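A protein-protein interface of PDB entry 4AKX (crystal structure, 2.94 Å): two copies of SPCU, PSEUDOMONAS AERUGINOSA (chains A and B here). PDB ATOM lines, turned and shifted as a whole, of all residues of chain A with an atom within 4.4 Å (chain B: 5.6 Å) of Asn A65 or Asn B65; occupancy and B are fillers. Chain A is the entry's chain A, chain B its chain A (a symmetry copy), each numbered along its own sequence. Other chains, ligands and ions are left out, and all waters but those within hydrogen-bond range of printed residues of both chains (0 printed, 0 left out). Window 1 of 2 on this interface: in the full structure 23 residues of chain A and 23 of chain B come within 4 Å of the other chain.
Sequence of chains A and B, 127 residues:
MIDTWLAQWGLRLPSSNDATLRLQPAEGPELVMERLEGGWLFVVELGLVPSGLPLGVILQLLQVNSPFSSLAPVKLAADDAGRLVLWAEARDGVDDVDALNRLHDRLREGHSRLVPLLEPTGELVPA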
ATOM      1  N   LEU A  61     -21.274  11.851  19.579  1.00  0.00           N
ATOM      2  CA  LEU A  61     -22.680  11.547  19.371  1.00  0.00           C
ATOM      3  C   LEU A  61     -23.039  11.296  17.905  1.00  0.00           C
ATOM      4  O   LEU A  61     -23.437  10.206  17.531  1.00  0.00           O
ATOM      5  CB  LEU A  61     -23.561  12.624  19.959  1.00  0.00           C
ATOM      6  CG  LEU A  61     -23.498  12.786  21.483  1.00  0.00           C
ATOM      7  CD1 LEU A  61     -24.643  13.654  21.965  1.00  0.00           C
ATOM      8  CD2 LEU A  61     -23.571  11.430  22.147  1.00  0.00           C
ATOM      9  N   LEU A  62     -22.831  12.283  17.064  1.00  0.00           N
ATOM     10  CA  LEU A  62     -23.023  12.097  15.638  1.00  0.00           C
ATOM     11  C   LEU A  62     -22.308  10.877  15.064  1.00  0.00           C
ATOM     12  O   LEU A  62     -22.854  10.172  14.202  1.00  0.00           O
ATOM     13  CB  LEU A  62     -22.605  13.365  14.919  1.00  0.00           C
ATOM     14  CG  LEU A  62     -23.430  14.544  15.476  1.00  0.00           C
ATOM     15  CD1 LEU A  62     -22.920  15.889  15.004  1.00  0.00           C
ATOM     16  CD2 LEU A  62     -24.903  14.409  15.124  1.00  0.00           C
ATOM     17  N   GLN A  63     -21.103  10.597  15.552  1.00  0.00           N
ATOM     18  CA  GLN A  63     -20.350   9.483  14.996  1.00  0.00           C
ATOM     19  C   GLN A  63     -20.993   8.111  15.242  1.00  0.00           C
ATOM     20  O   GLN A  63     -20.805   7.201  14.443  1.00  0.00           O
ATOM     21  CB  GLN A  63     -18.898   9.519  15.447  1.00  0.00           C
ATOM     22  CG  GLN A  63     -18.115  10.681  14.842  1.00  0.00           C
ATOM     23  CD  GLN A  63     -16.689  10.763  15.346  1.00  0.00           C
ATOM     24  OE1 GLN A  63     -16.393  10.361  16.467  1.00  0.00           O
ATOM     25  NE2 GLN A  63     -15.793  11.284  14.512  1.00  0.00           N
ATOM     26  N   VAL A  64     -21.763   7.967  16.323  1.00  0.00           N
ATOM     27  CA  VAL A  64     -22.612   6.781  16.514  1.00  0.00           C
ATOM     28  C   VAL A  64     -23.493   6.434  15.290  1.00  0.00           C
ATOM     29  O   VAL A  64     -24.024   5.335  15.216  1.00  0.00           O
ATOM     30  CB  VAL A  64     -23.574   6.958  17.703  1.00  0.00           C
ATOM     31  CG1 VAL A  64     -24.457   5.717  17.886  1.00  0.00           C
ATOM     32  CG2 VAL A  64     -22.831   7.334  18.983  1.00  0.00           C
ATOM     33  N   ASN A  65     -23.689   7.347  14.347  1.00  0.00           N
ATOM     34  CA  ASN A  65     -24.604   7.024  13.253  1.00  0.00           C
ATOM     35  C   ASN A  65     -23.937   6.717  11.929  1.00  0.00           C
ATOM     36  O   ASN A  65     -24.608   6.645  10.879  1.00  0.00           O
ATOM     37  CB  ASN A  65     -25.671   8.101  13.065  1.00  0.00           C
ATOM     38  CG  ASN A  65     -26.583   8.211  14.248  1.00  0.00           C
ATOM     39  OD1 ASN A  65     -26.822   7.240  14.931  1.00  0.00           O
ATOM     40  ND2 ASN A  65     -27.052   9.404  14.528  1.00  0.00           N
ATOM     41  N   SER A  66     -22.619   6.538  11.947  1.00  0.00           N
ATOM     42  CA  SER A  66     -21.954   6.215  10.704  1.00  0.00           C
ATOM     43  C   SER A  66     -22.313   4.796  10.348  1.00  0.00           C
ATOM     44  O   SER A  66     -22.546   3.980  11.245  1.00  0.00           O
ATOM     45  CB  SER A  66     -20.461   6.455  10.773  1.00  0.00           C
ATOM     46  OG  SER A  66     -19.847   5.598  11.674  1.00  0.00           O
ATOM     47  N   PRO A  67     -22.494   4.522   9.052  1.00  0.00           N
ATOM     48  CA  PRO A  67     -23.036   3.241   8.653  1.00  0.00           C
ATOM     49  C   PRO A  67     -22.073   2.179   9.046  1.00  0.00           C
ATOM     50  O   PRO A  67     -22.397   0.984   8.981  1.00  0.00           O
ATOM     51  CB  PRO A  67     -23.090   3.327   7.139  1.00  0.00           C
ATOM     52  CG  PRO A  67     -22.065   4.314   6.789  1.00  0.00           C
ATOM     53  CD  PRO A  67     -22.041   5.312   7.910  1.00  0.00           C
ATOM     54  N   LYS A  75     -29.422   3.349  16.223  1.00  0.00           N
ATOM     55  CA  LYS A  75     -29.281   4.778  15.928  1.00  0.00           C
ATOM     56  C   LYS A  75     -29.453   5.671  17.127  1.00  0.00           C
ATOM     57  O   LYS A  75     -30.117   5.308  18.096  1.00  0.00           O
ATOM     58  CB  LYS A  75     -30.215   5.191  14.833  1.00  0.00           C
ATOM     59  CG  LYS A  75     -29.782   4.597  13.503  1.00  0.00           C
ATOM     60  CD  LYS A  75     -30.972   4.491  12.556  1.00  0.00           C
ATOM     61  CE  LYS A  75     -31.136   3.079  11.995  1.00  0.00           C
ATOM     62  NZ  LYS A  75     -31.956   2.241  12.918  1.00  0.00           N
ATOM     63  N   LEU A  76     -28.826   6.836  17.067  1.00  0.00           N
ATOM     64  CA  LEU A  76     -28.940   7.808  18.108  1.00  0.00           C
ATOM     65  C   LEU A  76     -29.771   8.968  17.587  1.00  0.00           C
ATOM     66  O   LEU A  76     -29.536   9.426  16.456  1.00  0.00           O
ATOM     67  CB  LEU A  76     -27.559   8.296  18.476  1.00  0.00           C
ATOM     68  CG  LEU A  76     -27.472   8.998  19.813  1.00  0.00           C
ATOM     69  CD1 LEU A  76     -26.053   8.949  20.327  1.00  0.00           C
ATOM     70  CD2 LEU A  76     -27.878  10.419  19.568  1.00  0.00           C
ATOM     71  N   ALA A  77     -30.754   9.418  18.385  1.00  0.00           N
ATOM     72  CA  ALA A  77     -31.636  10.514  17.977  1.00  0.00           C
ATOM     73  C   ALA A  77     -32.157  11.182  19.189  1.00  0.00           C
ATOM     74  O   ALA A  77     -31.855  10.763  20.315  1.00  0.00           O
ATOM     75  CB  ALA A  77     -32.804  10.008  17.150  1.00  0.00           C
ATOM     76  N   TRP A  87     -32.041   3.718  19.460  1.00  0.00           N
ATOM     77  CA  TRP A  87     -33.111   2.815  19.069  1.00  0.00           C
ATOM     78  C   TRP A  87     -32.709   1.941  17.961  1.00  0.00           C
ATOM     79  O   TRP A  87     -31.748   2.241  17.267  1.00  0.00           O
ATOM     80  CB  TRP A  87     -34.364   3.577  18.671  1.00  0.00           C
ATOM     81  CG  TRP A  87     -34.206   4.438  17.443  1.00  0.00           C
ATOM     82  CD1 TRP A  87     -33.689   5.733  17.383  1.00  0.00           C
ATOM     83  CD2 TRP A  87     -34.596   4.135  16.086  1.00  0.00           C
ATOM     84  NE1 TRP A  87     -33.737   6.229  16.101  1.00  0.00           N
ATOM     85  CE2 TRP A  87     -34.272   5.334  15.281  1.00  0.00           C
ATOM     86  CE3 TRP A  87     -35.155   3.046  15.461  1.00  0.00           C
ATOM     87  CZ2 TRP A  87     -34.503   5.395  13.924  1.00  0.00           C
ATOM     88  CZ3 TRP A  87     -35.392   3.119  14.060  1.00  0.00           C
ATOM     89  CH2 TRP A  87     -35.064   4.262  13.319  1.00  0.00           C
ATOM     90  N   LEU B  61     -30.766  18.703  14.798  1.00  0.00           N
ATOM     91  CA  LEU B  61     -29.910  17.687  14.208  1.00  0.00           C
ATOM     92  C   LEU B  61     -30.248  16.266  14.662  1.00  0.00           C
ATOM     93  O   LEU B  61     -30.654  15.431  13.871  1.00  0.00           O
ATOM     94  CB  LEU B  61     -28.452  17.994  14.457  1.00  0.00           C
ATOM     95  CG  LEU B  61     -27.914  19.273  13.805  1.00  0.00           C
ATOM     96  CD1 LEU B  61     -26.399  19.291  13.859  1.00  0.00           C
ATOM     97  CD2 LEU B  61     -28.374  19.351  12.367  1.00  0.00           C
ATOM     98  N   LEU B  62     -30.151  16.013  15.946  1.00  0.00           N
ATOM     99  CA  LEU B  62     -30.570  14.733  16.485  1.00  0.00           C
ATOM    100  C   LEU B  62     -31.973  14.304  16.062  1.00  0.00           C
ATOM    101  O   LEU B  62     -32.215  13.120  15.781  1.00  0.00           O
ATOM    102  CB  LEU B  62     -30.442  14.773  17.996  1.00  0.00           C
ATOM    103  CG  LEU B  62     -28.983  15.115  18.360  1.00  0.00           C
ATOM    104  CD1 LEU B  62     -28.804  15.422  19.831  1.00  0.00           C
ATOM    105  CD2 LEU B  62     -28.031  14.000  17.955  1.00  0.00           C
ATOM    106  N   GLN B  63     -32.897  15.257  15.981  1.00  0.00           N
ATOM    107  CA  GLN B  63     -34.266  14.895  15.644  1.00  0.00           C
ATOM    108  C   GLN B  63     -34.431  14.331  14.226  1.00  0.00           C
ATOM    109  O   GLN B  63     -35.331  13.533  13.992  1.00  0.00           O
ATOM    110  CB  GLN B  63     -35.223  16.047  15.912  1.00  0.00           C
ATOM    111  CG  GLN B  63     -35.398  16.342  17.399  1.00  0.00           C
ATOM    112  CD  GLN B  63     -36.292  17.536  17.666  1.00  0.00           C
ATOM    113  OE1 GLN B  63     -36.371  18.457  16.859  1.00  0.00           O
ATOM    114  NE2 GLN B  63     -36.976  17.521  18.807  1.00  0.00           N
ATOM    115  N   VAL B  64     -33.558  14.720  13.293  1.00  0.00           N
ATOM    116  CA  VAL B  64     -33.480  14.056  11.983  1.00  0.00           C
ATOM    117  C   VAL B  64     -33.389  12.514  12.064  1.00  0.00           C
ATOM    118  O   VAL B  64     -33.596  11.839  11.065  1.00  0.00           O
ATOM    119  CB  VAL B  64     -32.251  14.522  11.184  1.00  0.00           C
ATOM    120  CG1 VAL B  64     -32.180  13.817   9.823  1.00  0.00           C
ATOM    121  CG2 VAL B  64     -32.202  16.043  11.051  1.00  0.00           C
ATOM    122  N   ASN B  65     -33.051  11.939  13.212  1.00  0.00           N
ATOM    123  CA  ASN B  65     -32.876  10.487  13.232  1.00  0.00           C
ATOM    124  C   ASN B  65     -33.993   9.717  13.903  1.00  0.00           C
ATOM    125  O   ASN B  65     -33.856   8.507  14.178  1.00  0.00           O
ATOM    126  CB  ASN B  65     -31.529  10.084  13.827  1.00  0.00           C
ATOM    127  CG  ASN B  65     -30.375  10.551  12.994  1.00  0.00           C
ATOM    128  OD1 ASN B  65     -30.492  10.669  11.794  1.00  0.00           O
ATOM    129  ND2 ASN B  65     -29.274  10.874  13.631  1.00  0.00           N
ATOM    130  N   SER B  66     -35.104  10.391  14.186  1.00  0.00           N
ATOM    131  CA  SER B  66     -36.201   9.678  14.802  1.00  0.00           C
ATOM    132  C   SER B  66     -36.809   8.780  13.755  1.00  0.00           C
ATOM    133  O   SER B  66     -36.776   9.115  12.567  1.00  0.00           O
ATOM    134  CB  SER B  66     -37.204  10.613  15.444  1.00  0.00           C
ATOM    135  OG  SER B  66     -37.848  11.398  14.498  1.00  0.00           O
ATOM    136  N   PRO B  67     -37.242   7.582  14.161  1.00  0.00           N
ATOM    137  CA  PRO B  67     -37.647   6.593  13.186  1.00  0.00           C
ATOM    138  C   PRO B  67     -38.839   7.105  12.461  1.00  0.00           C
ATOM    139  O   PRO B  67     -39.256   6.522  11.450  1.00  0.00           O
ATOM    140  CB  PRO B  67     -38.055   5.399  14.030  1.00  0.00           C
ATOM    141  CG  PRO B  67     -38.428   5.974  15.325  1.00  0.00           C
ATOM    142  CD  PRO B  67     -37.539   7.165  15.529  1.00  0.00           C
ATOM    143  N   SER B  69     -39.146  10.507  11.491  1.00  0.00           N
ATOM    144  CA  SER B  69     -38.850  11.728  10.771  1.00  0.00           C
ATOM    145  C   SER B  69     -39.434  11.716   9.368  1.00  0.00           C
ATOM    146  O   SER B  69     -39.619  10.662   8.764  1.00  0.00           O
ATOM    147  CB  SER B  69     -37.348  11.925  10.691  1.00  0.00           C
ATOM    148  OG  SER B  69     -36.991  12.358   9.392  1.00  0.00           O
ATOM    149  N   VAL B  74     -33.205   8.281   5.533  1.00  0.00           N
ATOM    150  CA  VAL B  74     -31.929   9.026   5.533  1.00  0.00           C
ATOM    151  C   VAL B  74     -31.463   9.295   6.953  1.00  0.00           C
ATOM    152  O   VAL B  74     -32.268   9.711   7.800  1.00  0.00           O
ATOM    153  CB  VAL B  74     -32.100  10.407   4.897  1.00  0.00           C
ATOM    154  CG1 VAL B  74     -31.032  11.361   5.414  1.00  0.00           C
ATOM    155  CG2 VAL B  74     -32.115  10.316   3.367  1.00  0.00           C
ATOM    156  N   LYS B  75     -30.164   9.114   7.207  1.00  0.00           N
ATOM    157  CA  LYS B  75     -29.596   9.386   8.531  1.00  0.00           C
ATOM    158  C   LYS B  75     -28.586  10.501   8.547  1.00  0.00           C
ATOM    159  O   LYS B  75     -27.951  10.794   7.537  1.00  0.00           O
ATOM    160  CB  LYS B  75     -29.008   8.142   9.123  1.00  0.00           C
ATOM    161  CG  LYS B  75     -30.100   7.154   9.497  1.00  0.00           C
ATOM    162  CD  LYS B  75     -29.548   5.735   9.520  1.00  0.00           C
ATOM    163  CE  LYS B  75     -30.370   4.783   8.651  1.00  0.00           C
ATOM    164  NZ  LYS B  75     -29.886   4.813   7.239  1.00  0.00           N
ATOM    165  N   LEU B  76     -28.460  11.141   9.700  1.00  0.00           N
ATOM    166  CA  LEU B  76     -27.504  12.188   9.880  1.00  0.00           C
ATOM    167  C   LEU B  76     -26.403  11.675  10.793  1.00  0.00           C
ATOM    168  O   LEU B  76     -26.708  11.050  11.823  1.00  0.00           O
ATOM    169  CB  LEU B  76     -28.188  13.370  10.523  1.00  0.00           C
ATOM    170  CG  LEU B  76     -27.437  14.678  10.401  1.00  0.00           C
ATOM    171  CD1 LEU B  76     -28.393  15.835  10.559  1.00  0.00           C
ATOM    172  CD2 LEU B  76     -26.433  14.690  11.514  1.00  0.00           C
ATOM    173  N   ALA B  77     -25.137  11.903  10.405  1.00  0.00           N
ATOM    174  CA  ALA B  77     -23.994  11.432  11.192  1.00  0.00           C
ATOM    175  C   ALA B  77     -22.832  12.302  10.910  1.00  0.00           C
ATOM    176  O   ALA B  77     -22.923  13.225  10.089  1.00  0.00           O
ATOM    177  CB  ALA B  77     -23.635   9.999  10.845  1.00  0.00           C
ATOM    178  N   TRP B  87     -26.876  10.349   4.941  1.00  0.00           N
ATOM    179  CA  TRP B  87     -26.665   9.193   4.086  1.00  0.00           C
ATOM    180  C   TRP B  87     -27.812   8.279   4.112  1.00  0.00           C
ATOM    181  O   TRP B  87     -28.622   8.344   5.027  1.00  0.00           O
ATOM    182  CB  TRP B  87     -25.412   8.429   4.483  1.00  0.00           C
ATOM    183  CG  TRP B  87     -25.471   7.806   5.855  1.00  0.00           C
ATOM    184  CD1 TRP B  87     -25.189   8.426   7.073  1.00  0.00           C
ATOM    185  CD2 TRP B  87     -25.778   6.439   6.200  1.00  0.00           C
ATOM    186  NE1 TRP B  87     -25.304   7.541   8.120  1.00  0.00           N
ATOM    187  CE2 TRP B  87     -25.644   6.339   7.671  1.00  0.00           C
ATOM    188  CE3 TRP B  87     -26.140   5.319   5.490  1.00  0.00           C
ATOM    189  CZ2 TRP B  87     -25.876   5.166   8.355  1.00  0.00           C
ATOM    190  CZ3 TRP B  87     -26.377   4.112   6.204  1.00  0.00           C
ATOM    191  CH2 TRP B  87     -26.254   4.049   7.599  1.00  0.00           C
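The backbone carbonyl oxygen (O) of Leu B76 lies within hydrogen-bond range of the side-chain amide nitrogen (ND2) of Asn A65 (3.2 Å). ND2 of Asn B65 lies close to ND2 of Asn A65 (2.8 Å). The indole nitrogen of Trp A87 lies within hydrogen-bond range of the backbone carbonyl oxygen of Asn B65 (3.0 Å). The side-chain amide nitrogen (ND2) of Asn B65 is in hydrogen-bond range of the backbone carbonyl oxygen (O) of Leu A76 (3.2 Å). O of Asn A65 is in hydrogen-bond range of NE1 of Trp B87 (3.0 Å).
O of Trp B87 lies within hydrogen-bond range of N of Lys B75 (2.8 Å). The backbone carbonyl oxygen (O) of Gln A63 sits at hydrogen-bond distance from the side-chain hydroxyl (OG) of Ser A66 (3.3 Å). The backbone NH (N) of Ser B69 sits at hydrogen-bond distance from the side-chain hydroxyl (OG) of Ser B66, 3.4 Å away. N of Leu A76 sits at hydrogen-bond distance from OD1 of Asn A65 (3.0 Å). N of Lys A75 is in hydrogen-bond range of O of Trp A87 (2.8 Å). The side-chain amide oxygen of Asn B65 sits at hydrogen-bond distance from the backbone NH of Leu B76.
Leu A62 touches Leu B76. Ala B77 touches Leu A62 (CB to O, 3.5 Å). CB of Ala B77 touches C of Asn A65, 3.5 Å away. CB of Ala B77 touches N of Ser A66, 3.8 Å away. Lys A75 touches Lys B75 (CD to CD, 3.6 Å). Leu B62 touches Leu A76. CB of Ala A77 touches O of Leu B62, at 3.5 Å. C of Asn B65 touches CB of Ala A77, at 3.5 Å. Ser B66 touches Ala A77. Trp A87 touches Pro B67 (CH2 to CB, 3.3 Å).
Of the printed residues of chain B, Asn A65 touches Asn B65 (2.8 Å), Leu B76 (3.2 Å), Ala B77 (3.5 Å) and Trp B87 (3.0 Å). Printed residues of chain B within 4 Å of Ala A77: Leu B62, Asn B65 and Ser B66. Of the printed residues of chain B, Leu A62 touches Leu B76 and Ala B77. The nearest residue of chain B that does not touch Asn A65 is Lys B75 (5.0 Å). The nearest printed residue of chain A that does not touch Lys B75 is Asn A65 (5.0 Å).
Printed residues of chain B that touch a printed residue of chain A: Leu B62, Asn B65, Ser B66, Pro B67, Lys B75, Leu B76, Ala B77 and Trp B87. Hydrophobic or aromatic side chains of chain A that line the printed part of chain B: Leu A62, Pro A67, Leu A76, Ala A77 and Trp A87. Among the printed residues, 16 pairs touch across the chains. Among the printed residues, no Asp or Glu carboxylate lies within 4 Å of a Lys or Arg side-chain nitrogen of the other chain.
Asn A65 touches its own counterpart, Asn B65. Asn A65 touches Leu B76, and with the chains exchanged Leu A76 touches Asn B65. Asn A65 touches Trp B87, and with the chains exchanged Trp A87 touches Asn B65. Lys B75 touches its own counterpart, Lys A75. Positions printed for both chains: 61, 62, 63, 64, 65, 66, 67, 75, 76, 77 and 87. Of the 16 pairs that touch across the chains among the printed residues, 16 have their exchanged pair printed and touching as well.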
